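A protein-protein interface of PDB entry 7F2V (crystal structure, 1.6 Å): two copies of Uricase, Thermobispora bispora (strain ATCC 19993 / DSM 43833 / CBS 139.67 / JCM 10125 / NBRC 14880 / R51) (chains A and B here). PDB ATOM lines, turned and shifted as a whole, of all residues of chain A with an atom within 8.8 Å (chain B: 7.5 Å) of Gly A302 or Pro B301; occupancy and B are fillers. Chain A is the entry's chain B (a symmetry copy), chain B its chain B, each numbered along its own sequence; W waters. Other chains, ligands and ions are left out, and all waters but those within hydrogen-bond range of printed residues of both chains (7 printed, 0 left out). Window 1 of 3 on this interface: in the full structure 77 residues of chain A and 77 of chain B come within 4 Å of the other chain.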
ATOM      1  N   ARG A  10     -21.399 -25.895  15.612  1.00  0.00           N
ATOM      2  CA  ARG A  10     -21.169 -26.864  16.669  1.00  0.00           C
ATOM      3  C   ARG A  10     -22.167 -26.641  17.800  1.00  0.00           C
ATOM      4  O   ARG A  10     -22.577 -25.514  18.080  1.00  0.00           O
ATOM      5  CB  ARG A  10     -19.740 -26.731  17.201  1.00  0.00           C
ATOM      6  CG  ARG A  10     -19.446 -25.369  17.827  1.00  0.00           C
ATOM      7  CD  ARG A  10     -18.094 -25.358  18.527  1.00  0.00           C
ATOM      8  NE  ARG A  10     -16.987 -25.337  17.575  1.00  0.00           N
ATOM      9  CZ  ARG A  10     -15.707 -25.455  17.921  1.00  0.00           C
ATOM     10  NH1 ARG A  10     -15.379 -25.609  19.199  1.00  0.00           N
ATOM     11  NH2 ARG A  10     -14.759 -25.422  16.987  1.00  0.00           N
ATOM     12  N   GLN A  12     -23.748 -28.801  21.664  1.00  0.00           N
ATOM     13  CA  GLN A  12     -23.818 -29.969  22.531  1.00  0.00           C
ATOM     14  C   GLN A  12     -24.733 -29.626  23.691  1.00  0.00           C
ATOM     15  O   GLN A  12     -24.943 -28.453  24.005  1.00  0.00           O
ATOM     16  CB  GLN A  12     -22.437 -30.387  23.047  1.00  0.00           C
ATOM     17  CG  GLN A  12     -21.780 -29.362  23.940  1.00  0.00           C
ATOM     18  CD  GLN A  12     -20.362 -29.762  24.317  1.00  0.00           C
ATOM     19  OE1 GLN A  12     -19.691 -30.471  23.573  1.00  0.00           O
ATOM     20  NE2 GLN A  12     -19.901 -29.295  25.470  1.00  0.00           N
ATOM     21  N   ARG A  42     -23.617 -34.911  21.448  1.00  0.00           N
ATOM     22  CA  ARG A  42     -23.470 -34.254  20.163  1.00  0.00           C
ATOM     23  C   ARG A  42     -24.166 -35.096  19.106  1.00  0.00           C
ATOM     24  O   ARG A  42     -24.280 -36.316  19.249  1.00  0.00           O
ATOM     25  CB  ARG A  42     -21.992 -34.074  19.787  1.00  0.00           C
ATOM     26  CG  ARG A  42     -21.240 -33.176  20.761  1.00  0.00           C
ATOM     27  CD  ARG A  42     -19.853 -33.677  21.034  1.00  0.00           C
ATOM     28  NE  ARG A  42     -19.133 -32.815  21.968  1.00  0.00           N
ATOM     29  CZ  ARG A  42     -17.875 -33.029  22.336  1.00  0.00           C
ATOM     30  NH1 ARG A  42     -17.217 -34.079  21.847  1.00  0.00           N
ATOM     31  NH2 ARG A  42     -17.283 -32.205  23.187  1.00  0.00           N
ATOM     32  N   ARG A 101     -19.784 -36.824  25.470  1.00  0.00           N
ATOM     33  CA  ARG A 101     -18.673 -36.455  26.332  1.00  0.00           C
ATOM     34  C   ARG A 101     -19.166 -36.536  27.769  1.00  0.00           C
ATOM     35  O   ARG A 101     -20.145 -35.873  28.122  1.00  0.00           O
ATOM     36  CB  ARG A 101     -18.175 -35.048  26.007  1.00  0.00           C
ATOM     37  CG  ARG A 101     -17.046 -34.550  26.926  1.00  0.00           C
ATOM     38  CD  ARG A 101     -16.774 -33.075  26.665  1.00  0.00           C
ATOM     39  NE  ARG A 101     -15.630 -32.526  27.404  1.00  0.00           N
ATOM     40  CZ  ARG A 101     -15.697 -32.033  28.640  1.00  0.00           C
ATOM     41  NH1 ARG A 101     -16.848 -32.031  29.309  1.00  0.00           N
ATOM     42  NH2 ARG A 101     -14.617 -31.527  29.212  1.00  0.00           N
ATOM     43  N   VAL A 134     -12.291 -37.131  31.577  1.00  0.00           N
ATOM     44  CA  VAL A 134     -13.103 -36.650  30.456  1.00  0.00           C
ATOM     45  C   VAL A 134     -13.088 -37.755  29.416  1.00  0.00           C
ATOM     46  O   VAL A 134     -12.049 -38.018  28.788  1.00  0.00           O
ATOM     47  CB  VAL A 134     -12.583 -35.338  29.850  1.00  0.00           C
ATOM     48  CG1 VAL A 134     -13.501 -34.901  28.674  1.00  0.00           C
ATOM     49  CG2 VAL A 134     -12.484 -34.266  30.911  1.00  0.00           C
ATOM     50  N   HIS A 189      -3.426 -27.879  37.906  1.00  0.00           N
ATOM     51  CA  HIS A 189      -4.501 -28.446  37.112  1.00  0.00           C
ATOM     52  C   HIS A 189      -3.839 -29.160  35.944  1.00  0.00           C
ATOM     53  O   HIS A 189      -2.998 -28.567  35.261  1.00  0.00           O
ATOM     54  CB  HIS A 189      -5.466 -27.361  36.627  1.00  0.00           C
ATOM     55  CG  HIS A 189      -6.457 -27.843  35.615  1.00  0.00           C
ATOM     56  ND1 HIS A 189      -7.433 -28.770  35.912  1.00  0.00           N
ATOM     57  CD2 HIS A 189      -6.632 -27.517  34.310  1.00  0.00           C
ATOM     58  CE1 HIS A 189      -8.150 -29.017  34.830  1.00  0.00           C
ATOM     59  NE2 HIS A 189      -7.692 -28.262  33.847  1.00  0.00           N
ATOM     60  N   ARG A 191      -4.408 -32.544  32.832  1.00  0.00           N
ATOM     61  CA  ARG A 191      -5.078 -33.678  32.207  1.00  0.00           C
ATOM     62  C   ARG A 191      -4.107 -34.385  31.272  1.00  0.00           C
ATOM     63  O   ARG A 191      -3.324 -33.731  30.578  1.00  0.00           O
ATOM     64  CB  ARG A 191      -6.305 -33.257  31.389  1.00  0.00           C
ATOM     65  CG  ARG A 191      -7.362 -32.517  32.168  1.00  0.00           C
ATOM     66  CD  ARG A 191      -8.602 -32.327  31.301  1.00  0.00           C
ATOM     67  NE  ARG A 191      -9.379 -31.170  31.737  1.00  0.00           N
ATOM     68  CZ  ARG A 191     -10.377 -31.238  32.607  1.00  0.00           C
ATOM     69  NH1 ARG A 191     -10.708 -32.407  33.143  1.00  0.00           N
ATOM     70  NH2 ARG A 191     -11.032 -30.142  32.950  1.00  0.00           N
ATOM     71  N   LEU A 280       0.470 -17.294  35.195  1.00  0.00           N
ATOM     72  CA  LEU A 280      -0.240 -18.498  34.775  1.00  0.00           C
ATOM     73  C   LEU A 280       0.587 -19.154  33.685  1.00  0.00           C
ATOM     74  O   LEU A 280       0.711 -18.609  32.587  1.00  0.00           O
ATOM     75  CB  LEU A 280      -1.660 -18.191  34.297  1.00  0.00           C
ATOM     76  CG  LEU A 280      -2.531 -19.396  33.899  1.00  0.00           C
ATOM     77  CD1 LEU A 280      -2.627 -20.416  35.033  1.00  0.00           C
ATOM     78  CD2 LEU A 280      -3.917 -18.920  33.487  1.00  0.00           C
ATOM     79  N   GLU A 282       1.406 -22.424  31.362  1.00  0.00           N
ATOM     80  CA  GLU A 282       0.666 -23.546  30.787  1.00  0.00           C
ATOM     81  C   GLU A 282       1.502 -24.251  29.727  1.00  0.00           C
ATOM     82  O   GLU A 282       2.067 -23.598  28.846  1.00  0.00           O
ATOM     83  CB  GLU A 282      -0.655 -23.042  30.209  1.00  0.00           C
ATOM     84  CG  GLU A 282      -1.300 -22.012  31.167  1.00  0.00           C
ATOM     85  CD  GLU A 282      -2.740 -21.682  30.865  1.00  0.00           C
ATOM     86  OE1 GLU A 282      -2.971 -20.716  30.110  1.00  0.00           O
ATOM     87  OE2 GLU A 282      -3.639 -22.358  31.418  1.00  0.00           O
ATOM     88  N   TRP A 297     -10.151 -33.722  23.137  1.00  0.00           N
ATOM     89  CA  TRP A 297     -10.036 -32.438  23.810  1.00  0.00           C
ATOM     90  C   TRP A 297     -11.128 -31.459  23.423  1.00  0.00           C
ATOM     91  O   TRP A 297     -11.162 -30.346  23.964  1.00  0.00           O
ATOM     92  CB  TRP A 297      -8.676 -31.816  23.504  1.00  0.00           C
ATOM     93  CG  TRP A 297      -7.526 -32.614  24.044  1.00  0.00           C
ATOM     94  CD1 TRP A 297      -6.801 -33.557  23.379  1.00  0.00           C
ATOM     95  CD2 TRP A 297      -6.967 -32.534  25.366  1.00  0.00           C
ATOM     96  NE1 TRP A 297      -5.818 -34.067  24.202  1.00  0.00           N
ATOM     97  CE2 TRP A 297      -5.902 -33.453  25.426  1.00  0.00           C
ATOM     98  CE3 TRP A 297      -7.262 -31.768  26.499  1.00  0.00           C
ATOM     99  CZ2 TRP A 297      -5.134 -33.633  26.576  1.00  0.00           C
ATOM    100  CZ3 TRP A 297      -6.492 -31.946  27.642  1.00  0.00           C
ATOM    101  CH2 TRP A 297      -5.448 -32.864  27.674  1.00  0.00           C
ATOM    102  N   LEU A 298     -12.021 -31.839  22.512  1.00  0.00           N
ATOM    103  CA  LEU A 298     -13.003 -30.894  22.010  1.00  0.00           C
ATOM    104  C   LEU A 298     -13.928 -30.452  23.133  1.00  0.00           C
ATOM    105  O   LEU A 298     -14.540 -31.281  23.815  1.00  0.00           O
ATOM    106  CB  LEU A 298     -13.802 -31.526  20.872  1.00  0.00           C
ATOM    107  CG  LEU A 298     -14.679 -30.564  20.067  1.00  0.00           C
ATOM    108  CD1 LEU A 298     -13.841 -29.641  19.189  1.00  0.00           C
ATOM    109  CD2 LEU A 298     -15.674 -31.354  19.233  1.00  0.00           C
ATOM    110  N   ALA A 299     -14.010 -29.128  23.325  1.00  0.00           N
ATOM    111  CA  ALA A 299     -14.810 -28.478  24.360  1.00  0.00           C
ATOM    112  C   ALA A 299     -14.280 -28.749  25.764  1.00  0.00           C
ATOM    113  O   ALA A 299     -15.030 -28.658  26.740  1.00  0.00           O
ATOM    114  CB  ALA A 299     -16.293 -28.867  24.259  1.00  0.00           C
ATOM    115  N   THR A 300     -12.987 -29.095  25.889  1.00  0.00           N
ATOM    116  CA  THR A 300     -12.284 -29.088  27.169  1.00  0.00           C
ATOM    117  C   THR A 300     -11.369 -27.877  27.205  1.00  0.00           C
ATOM    118  O   THR A 300     -10.594 -27.688  26.256  1.00  0.00           O
ATOM    119  CB  THR A 300     -11.455 -30.371  27.344  1.00  0.00           C
ATOM    120  OG1 THR A 300     -12.321 -31.501  27.478  1.00  0.00           O
ATOM    121  CG2 THR A 300     -10.576 -30.272  28.582  1.00  0.00           C
ATOM    122  N   PRO A 301     -11.400 -27.035  28.254  1.00  0.00           N
ATOM    123  CA  PRO A 301     -12.189 -27.170  29.486  1.00  0.00           C
ATOM    124  C   PRO A 301     -13.662 -26.795  29.331  1.00  0.00           C
ATOM    125  O   PRO A 301     -14.468 -27.124  30.207  1.00  0.00           O
ATOM    126  CB  PRO A 301     -11.489 -26.207  30.449  1.00  0.00           C
ATOM    127  CG  PRO A 301     -10.910 -25.159  29.572  1.00  0.00           C
ATOM    128  CD  PRO A 301     -10.485 -25.879  28.317  1.00  0.00           C
ATOM    129  N   GLY A 302     -14.006 -26.127  28.234  1.00  0.00           N
ATOM    130  CA  GLY A 302     -15.385 -25.739  28.018  1.00  0.00           C
ATOM    131  C   GLY A 302     -15.645 -25.412  26.564  1.00  0.00           C
ATOM    132  O   GLY A 302     -14.739 -25.404  25.729  1.00  0.00           O
ATOM    133  N   PHE A 303     -16.917 -25.094  26.293  1.00  0.00           N
ATOM    134  CA  PHE A 303     -17.431 -24.931  24.930  1.00  0.00           C
ATOM    135  C   PHE A 303     -17.056 -23.581  24.337  1.00  0.00           C
ATOM    136  O   PHE A 303     -16.781 -23.483  23.136  1.00  0.00           O
ATOM    137  CB  PHE A 303     -18.953 -25.093  24.961  1.00  0.00           C
ATOM    138  CG  PHE A 303     -19.618 -24.928  23.634  1.00  0.00           C
ATOM    139  CD1 PHE A 303     -19.677 -25.988  22.742  1.00  0.00           C
ATOM    140  CD2 PHE A 303     -20.236 -23.727  23.293  1.00  0.00           C
ATOM    141  CE1 PHE A 303     -20.321 -25.850  21.519  1.00  0.00           C
ATOM    142  CE2 PHE A 303     -20.864 -23.582  22.066  1.00  0.00           C
ATOM    143  CZ  PHE A 303     -20.907 -24.648  21.183  1.00  0.00           C
ATOM    144  N   CYS A 304     -17.082 -22.533  25.153  1.00  0.00           N
ATOM    145  CA  CYS A 304     -16.764 -21.182  24.701  1.00  0.00           C
ATOM    146  C   CYS A 304     -16.488 -20.261  25.884  1.00  0.00           C
ATOM    147  O   CYS A 304     -16.528 -20.676  27.048  1.00  0.00           O
ATOM    148  CB  CYS A 304     -17.902 -20.615  23.841  1.00  0.00           C
ATOM    149  SG  CYS A 304     -19.440 -20.188  24.741  1.00  0.00           S
ATOM    150  OXT CYS A 304     -16.203 -19.083  25.677  1.00  0.00           O
ATOM    151  N   ARG B 101      -2.287 -13.452  23.428  1.00  0.00           N
ATOM    152  CA  ARG B 101      -3.714 -13.485  23.704  1.00  0.00           C
ATOM    153  C   ARG B 101      -3.960 -12.618  24.929  1.00  0.00           C
ATOM    154  O   ARG B 101      -3.374 -12.865  25.986  1.00  0.00           O
ATOM    155  CB  ARG B 101      -4.189 -14.916  23.947  1.00  0.00           C
ATOM    156  CG  ARG B 101      -5.677 -15.033  24.321  1.00  0.00           C
ATOM    157  CD  ARG B 101      -5.997 -16.457  24.752  1.00  0.00           C
ATOM    158  NE  ARG B 101      -7.419 -16.711  25.014  1.00  0.00           N
ATOM    159  CZ  ARG B 101      -8.020 -16.494  26.184  1.00  0.00           C
ATOM    160  NH1 ARG B 101      -7.342 -15.993  27.214  1.00  0.00           N
ATOM    161  NH2 ARG B 101      -9.301 -16.785  26.335  1.00  0.00           N
ATOM    162  N   VAL B 134     -11.658 -11.149  24.080  1.00  0.00           N
ATOM    163  CA  VAL B 134     -10.486 -12.013  23.907  1.00  0.00           C
ATOM    164  C   VAL B 134      -9.847 -11.603  22.593  1.00  0.00           C
ATOM    165  O   VAL B 134     -10.412 -11.844  21.513  1.00  0.00           O
ATOM    166  CB  VAL B 134     -10.833 -13.508  23.889  1.00  0.00           C
ATOM    167  CG1 VAL B 134      -9.537 -14.347  23.705  1.00  0.00           C
ATOM    168  CG2 VAL B 134     -11.576 -13.896  25.147  1.00  0.00           C
ATOM    169  N   HIS B 189     -23.671 -17.054  29.085  1.00  0.00           N
ATOM    170  CA  HIS B 189     -22.280 -16.823  28.740  1.00  0.00           C
ATOM    171  C   HIS B 189     -22.196 -16.902  27.224  1.00  0.00           C
ATOM    172  O   HIS B 189     -22.684 -17.871  26.633  1.00  0.00           O
ATOM    173  CB  HIS B 189     -21.364 -17.856  29.403  1.00  0.00           C
ATOM    174  CG  HIS B 189     -19.954 -17.820  28.906  1.00  0.00           C
ATOM    175  ND1 HIS B 189     -19.118 -16.743  29.113  1.00  0.00           N
ATOM    176  CD2 HIS B 189     -19.225 -18.734  28.218  1.00  0.00           C
ATOM    177  CE1 HIS B 189     -17.945 -16.981  28.554  1.00  0.00           C
ATOM    178  NE2 HIS B 189     -17.980 -18.186  28.013  1.00  0.00           N
ATOM    179  N   ARG B 191     -19.741 -15.523  23.546  1.00  0.00           N
ATOM    180  CA  ARG B 191     -18.701 -14.782  22.841  1.00  0.00           C
ATOM    181  C   ARG B 191     -18.998 -14.792  21.348  1.00  0.00           C
ATOM    182  O   ARG B 191     -19.439 -15.811  20.809  1.00  0.00           O
ATOM    183  CB  ARG B 191     -17.306 -15.382  23.053  1.00  0.00           C
ATOM    184  CG  ARG B 191     -16.865 -15.467  24.493  1.00  0.00           C
ATOM    185  CD  ARG B 191     -15.403 -15.893  24.558  1.00  0.00           C
ATOM    186  NE  ARG B 191     -15.100 -16.546  25.829  1.00  0.00           N
ATOM    187  CZ  ARG B 191     -14.640 -15.907  26.895  1.00  0.00           C
ATOM    188  NH1 ARG B 191     -14.444 -14.594  26.844  1.00  0.00           N
ATOM    189  NH2 ARG B 191     -14.390 -16.572  28.009  1.00  0.00           N
ATOM    190  N   ARG B 246     -21.098 -17.895  19.834  1.00  0.00           N
ATOM    191  CA  ARG B 246     -21.261 -19.086  20.655  1.00  0.00           C
ATOM    192  C   ARG B 246     -21.988 -18.713  21.937  1.00  0.00           C
ATOM    193  O   ARG B 246     -21.692 -17.683  22.558  1.00  0.00           O
ATOM    194  CB  ARG B 246     -19.906 -19.713  21.003  1.00  0.00           C
ATOM    195  CG  ARG B 246     -19.111 -20.176  19.789  1.00  0.00           C
ATOM    196  CD  ARG B 246     -18.030 -21.123  20.241  1.00  0.00           C
ATOM    197  NE  ARG B 246     -17.086 -21.388  19.167  1.00  0.00           N
ATOM    198  CZ  ARG B 246     -15.903 -21.959  19.355  1.00  0.00           C
ATOM    199  NH1 ARG B 246     -15.517 -22.314  20.582  1.00  0.00           N
ATOM    200  NH2 ARG B 246     -15.111 -22.161  18.320  1.00  0.00           N
ATOM    201  N   SER B 248     -23.536 -20.371  25.674  1.00  0.00           N
ATOM    202  CA  SER B 248     -23.550 -21.463  26.631  1.00  0.00           C
ATOM    203  C   SER B 248     -24.492 -21.051  27.752  1.00  0.00           C
ATOM    204  O   SER B 248     -24.271 -20.028  28.405  1.00  0.00           O
ATOM    205  CB  SER B 248     -22.133 -21.743  27.156  1.00  0.00           C
ATOM    206  OG  SER B 248     -22.157 -22.595  28.296  1.00  0.00           O
ATOM    207  N   GLU B 282     -25.508 -25.693  24.850  1.00  0.00           N
ATOM    208  CA  GLU B 282     -24.435 -24.926  24.222  1.00  0.00           C
ATOM    209  C   GLU B 282     -24.554 -24.982  22.704  1.00  0.00           C
ATOM    210  O   GLU B 282     -24.716 -26.063  22.134  1.00  0.00           O
ATOM    211  CB  GLU B 282     -23.083 -25.462  24.693  1.00  0.00           C
ATOM    212  CG  GLU B 282     -23.127 -25.760  26.210  1.00  0.00           C
ATOM    213  CD  GLU B 282     -21.780 -25.991  26.848  1.00  0.00           C
ATOM    214  OE1 GLU B 282     -21.355 -27.162  26.906  1.00  0.00           O
ATOM    215  OE2 GLU B 282     -21.169 -25.009  27.331  1.00  0.00           O
ATOM    216  N   TRP B 297      -9.967 -18.631  18.731  1.00  0.00           N
ATOM    217  CA  TRP B 297     -10.569 -19.397  19.811  1.00  0.00           C
ATOM    218  C   TRP B 297      -9.574 -20.272  20.551  1.00  0.00           C
ATOM    219  O   TRP B 297      -9.960 -20.938  21.520  1.00  0.00           O
ATOM    220  CB  TRP B 297     -11.690 -20.273  19.258  1.00  0.00           C
ATOM    221  CG  TRP B 297     -12.833 -19.483  18.692  1.00  0.00           C
ATOM    222  CD1 TRP B 297     -13.011 -19.120  17.390  1.00  0.00           C
ATOM    223  CD2 TRP B 297     -13.960 -18.959  19.414  1.00  0.00           C
ATOM    224  NE1 TRP B 297     -14.185 -18.407  17.253  1.00  0.00           N
ATOM    225  CE2 TRP B 297     -14.783 -18.297  18.483  1.00  0.00           C
ATOM    226  CE3 TRP B 297     -14.353 -18.993  20.757  1.00  0.00           C
ATOM    227  CZ2 TRP B 297     -15.973 -17.669  18.851  1.00  0.00           C
ATOM    228  CZ3 TRP B 297     -15.541 -18.371  21.119  1.00  0.00           C
ATOM    229  CH2 TRP B 297     -16.332 -17.721  20.179  1.00  0.00           C
ATOM    230  N   LEU B 298      -8.312 -20.285  20.130  1.00  0.00           N
ATOM    231  CA  LEU B 298      -7.353 -21.204  20.718  1.00  0.00           C
ATOM    232  C   LEU B 298      -7.150 -20.881  22.190  1.00  0.00           C
ATOM    233  O   LEU B 298      -6.827 -19.744  22.550  1.00  0.00           O
ATOM    234  CB  LEU B 298      -6.028 -21.132  19.962  1.00  0.00           C
ATOM    235  CG  LEU B 298      -5.019 -22.234  20.290  1.00  0.00           C
ATOM    236  CD1 LEU B 298      -5.457 -23.582  19.729  1.00  0.00           C
ATOM    237  CD2 LEU B 298      -3.647 -21.846  19.766  1.00  0.00           C
ATOM    238  N   ALA B 299      -7.357 -21.897  23.038  1.00  0.00           N
ATOM    239  CA  ALA B 299      -7.248 -21.812  24.492  1.00  0.00           C
ATOM    240  C   ALA B 299      -8.340 -20.944  25.110  1.00  0.00           C
ATOM    241  O   ALA B 299      -8.167 -20.421  26.214  1.00  0.00           O
ATOM    242  CB  ALA B 299      -5.859 -21.324  24.930  1.00  0.00           C
ATOM    243  N   THR B 300      -9.472 -20.768  24.407  1.00  0.00           N
ATOM    244  CA  THR B 300     -10.694 -20.225  24.993  1.00  0.00           C
ATOM    245  C   THR B 300     -11.675 -21.365  25.197  1.00  0.00           C
ATOM    246  O   THR B 300     -11.921 -22.116  24.242  1.00  0.00           O
ATOM    247  CB  THR B 300     -11.315 -19.162  24.073  1.00  0.00           C
ATOM    248  OG1 THR B 300     -10.469 -18.011  24.008  1.00  0.00           O
ATOM    249  CG2 THR B 300     -12.683 -18.742  24.592  1.00  0.00           C
ATOM    250  N   PRO B 301     -12.268 -21.544  26.392  1.00  0.00           N
ATOM    251  CA  PRO B 301     -12.152 -20.693  27.584  1.00  0.00           C
ATOM    252  C   PRO B 301     -10.854 -20.883  28.365  1.00  0.00           C
ATOM    253  O   PRO B 301     -10.525 -20.045  29.212  1.00  0.00           O
ATOM    254  CB  PRO B 301     -13.354 -21.122  28.429  1.00  0.00           C
ATOM    255  CG  PRO B 301     -13.586 -22.539  28.055  1.00  0.00           C
ATOM    256  CD  PRO B 301     -13.255 -22.624  26.586  1.00  0.00           C
ATOM    257  N   GLY B 302     -10.125 -21.959  28.081  1.00  0.00           N
ATOM    258  CA  GLY B 302      -8.881 -22.204  28.781  1.00  0.00           C
ATOM    259  C   GLY B 302      -8.008 -23.183  28.028  1.00  0.00           C
ATOM    260  O   GLY B 302      -8.396 -23.741  27.000  1.00  0.00           O
ATOM    261  N   PHE B 303      -6.819 -23.411  28.601  1.00  0.00           N
ATOM    262  CA  PHE B 303      -5.747 -24.169  27.951  1.00  0.00           C
ATOM    263  C   PHE B 303      -5.978 -25.671  28.031  1.00  0.00           C
ATOM    264  O   PHE B 303      -5.658 -26.402  27.088  1.00  0.00           O
ATOM    265  CB  PHE B 303      -4.418 -23.802  28.617  1.00  0.00           C
ATOM    266  CG  PHE B 303      -3.231 -24.521  28.067  1.00  0.00           C
ATOM    267  CD1 PHE B 303      -2.605 -24.064  26.916  1.00  0.00           C
ATOM    268  CD2 PHE B 303      -2.701 -25.628  28.725  1.00  0.00           C
ATOM    269  CE1 PHE B 303      -1.482 -24.711  26.416  1.00  0.00           C
ATOM    270  CE2 PHE B 303      -1.592 -26.285  28.218  1.00  0.00           C
ATOM    271  CZ  PHE B 303      -0.983 -25.820  27.064  1.00  0.00           C
ATOM    272  N   CYS B 304      -6.494 -26.144  29.161  1.00  0.00           N
ATOM    273  CA  CYS B 304      -6.744 -27.566  29.370  1.00  0.00           C
ATOM    274  C   CYS B 304      -7.677 -27.788  30.554  1.00  0.00           C
ATOM    275  O   CYS B 304      -8.140 -26.839  31.199  1.00  0.00           O
ATOM    276  CB  CYS B 304      -5.426 -28.325  29.584  1.00  0.00           C
ATOM    277  SG  CYS B 304      -4.582 -28.015  31.180  1.00  0.00           S
ATOM    278  OXT CYS B 304      -7.993 -28.935  30.868  1.00  0.00           O
HETATM  279  O   HOH W   1     -27.366 -27.177  22.171  1.00  0.00           O
HETATM  280  O   HOH W   2      -6.242 -24.629  31.859  1.00  0.00           O
HETATM  281  O   HOH W   3      -6.175 -22.231  31.146  1.00  0.00           O
HETATM  282  O   HOH W   4     -19.592 -28.341  28.690  1.00  0.00           O
HETATM  283  O   HOH W   5     -18.857 -24.897  28.411  1.00  0.00           O
HETATM  284  O   HOH W   6     -12.484 -23.327  17.285  1.00  0.00           O
HETATM  285  O   HOH W   7     -18.801 -22.488  27.738  1.00  0.00           O
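His A189 touches Cys B304, and with the chains exchanged Cys A304 touches His B189. Glu A282 touches Phe B303, and with the chains exchanged Phe A303 touches Glu B282. Thr A300 touches Cys B304, and with the chains exchanged Cys A304 touches Thr B300. Pro A301 touches Cys B304, and with the chains exchanged Cys A304 touches Pro B301. 13 positions are printed for both chains. Of the 17 pairs that touch across the chains among the printed residues, 12 have their exchanged pair printed and touching as well.
Among the printed residues, pairs that only touch across the chains: Phe A303 with Glu B282 (3.2 Å), Glu A282 with Phe B303 (3.2 Å), Gly A302 with Pro B301 (3.3 Å), Pro A301 with Gly B302 (3.3 Å), Arg A10 with Arg B246 (3.4 Å), Pro A301 with Cys B304 (3.5 Å), Cys A304 with Pro B301 (3.5 Å), Cys A304 with Arg B246 (3.6 Å), Cys A304 with Thr B300 (3.7 Å), Thr A300 with Cys B304 (3.7 Å) and Cys A304 with Ser B248 (3.9 Å).
Water W5 bridges the side-chain carboxylate of Glu B282 (2.6 Å) and the backbone NH of Phe A303 (2.9 Å). Water W3 lies within hydrogen-bond range of OE2 of Glu A282 (2.6 Å) and N of Phe B303 (2.9 Å). Water W1 bridges the backbone carbonyl oxygen of Glu B282 and the backbone carbonyl oxygen of Gln A12. Water W2 lies within hydrogen-bond range of the chain-end carboxylate (O) of Cys B304 (3.0 Å) and the side-chain carboxylate (OE2) of Glu A282 (3.5 Å). Water W7 lies within hydrogen-bond range of O of Cys A304, OG of Ser B248 and OE2 of Glu B282. Water W6 bridges the guanidinium group (NH2) of Arg B246 and the guanidinium group (NH2) of Arg A10.
A ring nitrogen (NE2) of His B189 sits at hydrogen-bond distance from the chain-end carboxylate (O) of Cys A304 (3.0 Å). NE of Arg B191 is in salt-bridge range of OXT of Cys A304 (2.8 Å). NH1 of Arg B246 lies within hydrogen-bond range of O of Phe A303, 3.1 Å away. N of Glu B282 sits at hydrogen-bond distance from O of Gln A12 (2.9 Å). The chain-end carboxylate (O) of Cys B304 is in hydrogen-bond range of a ring nitrogen (NE2) of His A189 (3.0 Å). OXT of Cys B304 is in salt-bridge range of NE of Arg A191 (2.8 Å).
The side-chain hydroxyl of Thr B300 is in hydrogen-bond range of the guanidinium group of Arg B101 (2.9 Å). The backbone NH (N) of Ser B248 lies within hydrogen-bond range of the backbone carbonyl oxygen (O) of His B189, 2.8 Å away. O of Arg B191 is in hydrogen-bond range of N of Arg B246, at 2.8 Å. The side-chain hydroxyl (OG) of Ser B248 sits at hydrogen-bond distance from the side-chain carboxylate (OE2) of Glu B282, 2.8 Å away. The side-chain amide oxygen (OE1) of Gln A12 is in hydrogen-bond range of the guanidinium group (NE) of Arg A42, at 2.9 Å. The guanidinium group (NH2) of Arg A101 sits at hydrogen-bond distance from the side-chain hydroxyl (OG1) of Thr A300 (2.9 Å).
Printed residues of chain A within 4 Å of Pro B301: Gly A302 and Cys A304. Thr B300 touches just one residue of chain A: Cys A304 (3.7 Å). Of the printed residues of chain A, Gly B302 touches Pro A301 (3.3 Å). Printed residues of chain B within 4 Å of Thr A300: Cys B304 (3.7 Å). Printed residues of chain B within 4 Å of Gln A12: Glu B282. Of the printed residues of chain A, Ser B248 touches Cys A304. Of the printed residues of chain B, Arg A10 touches Arg B246. The nearest residue of chain B that does not touch Gly A302 is Thr B300 (4.6 Å).
Printed residues of chain A that touch a printed residue of chain B: Arg A10, Gln A12, His A189, Arg A191, Glu A282, Thr A300, Pro A301, Gly A302, Phe A303 and Cys A304.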
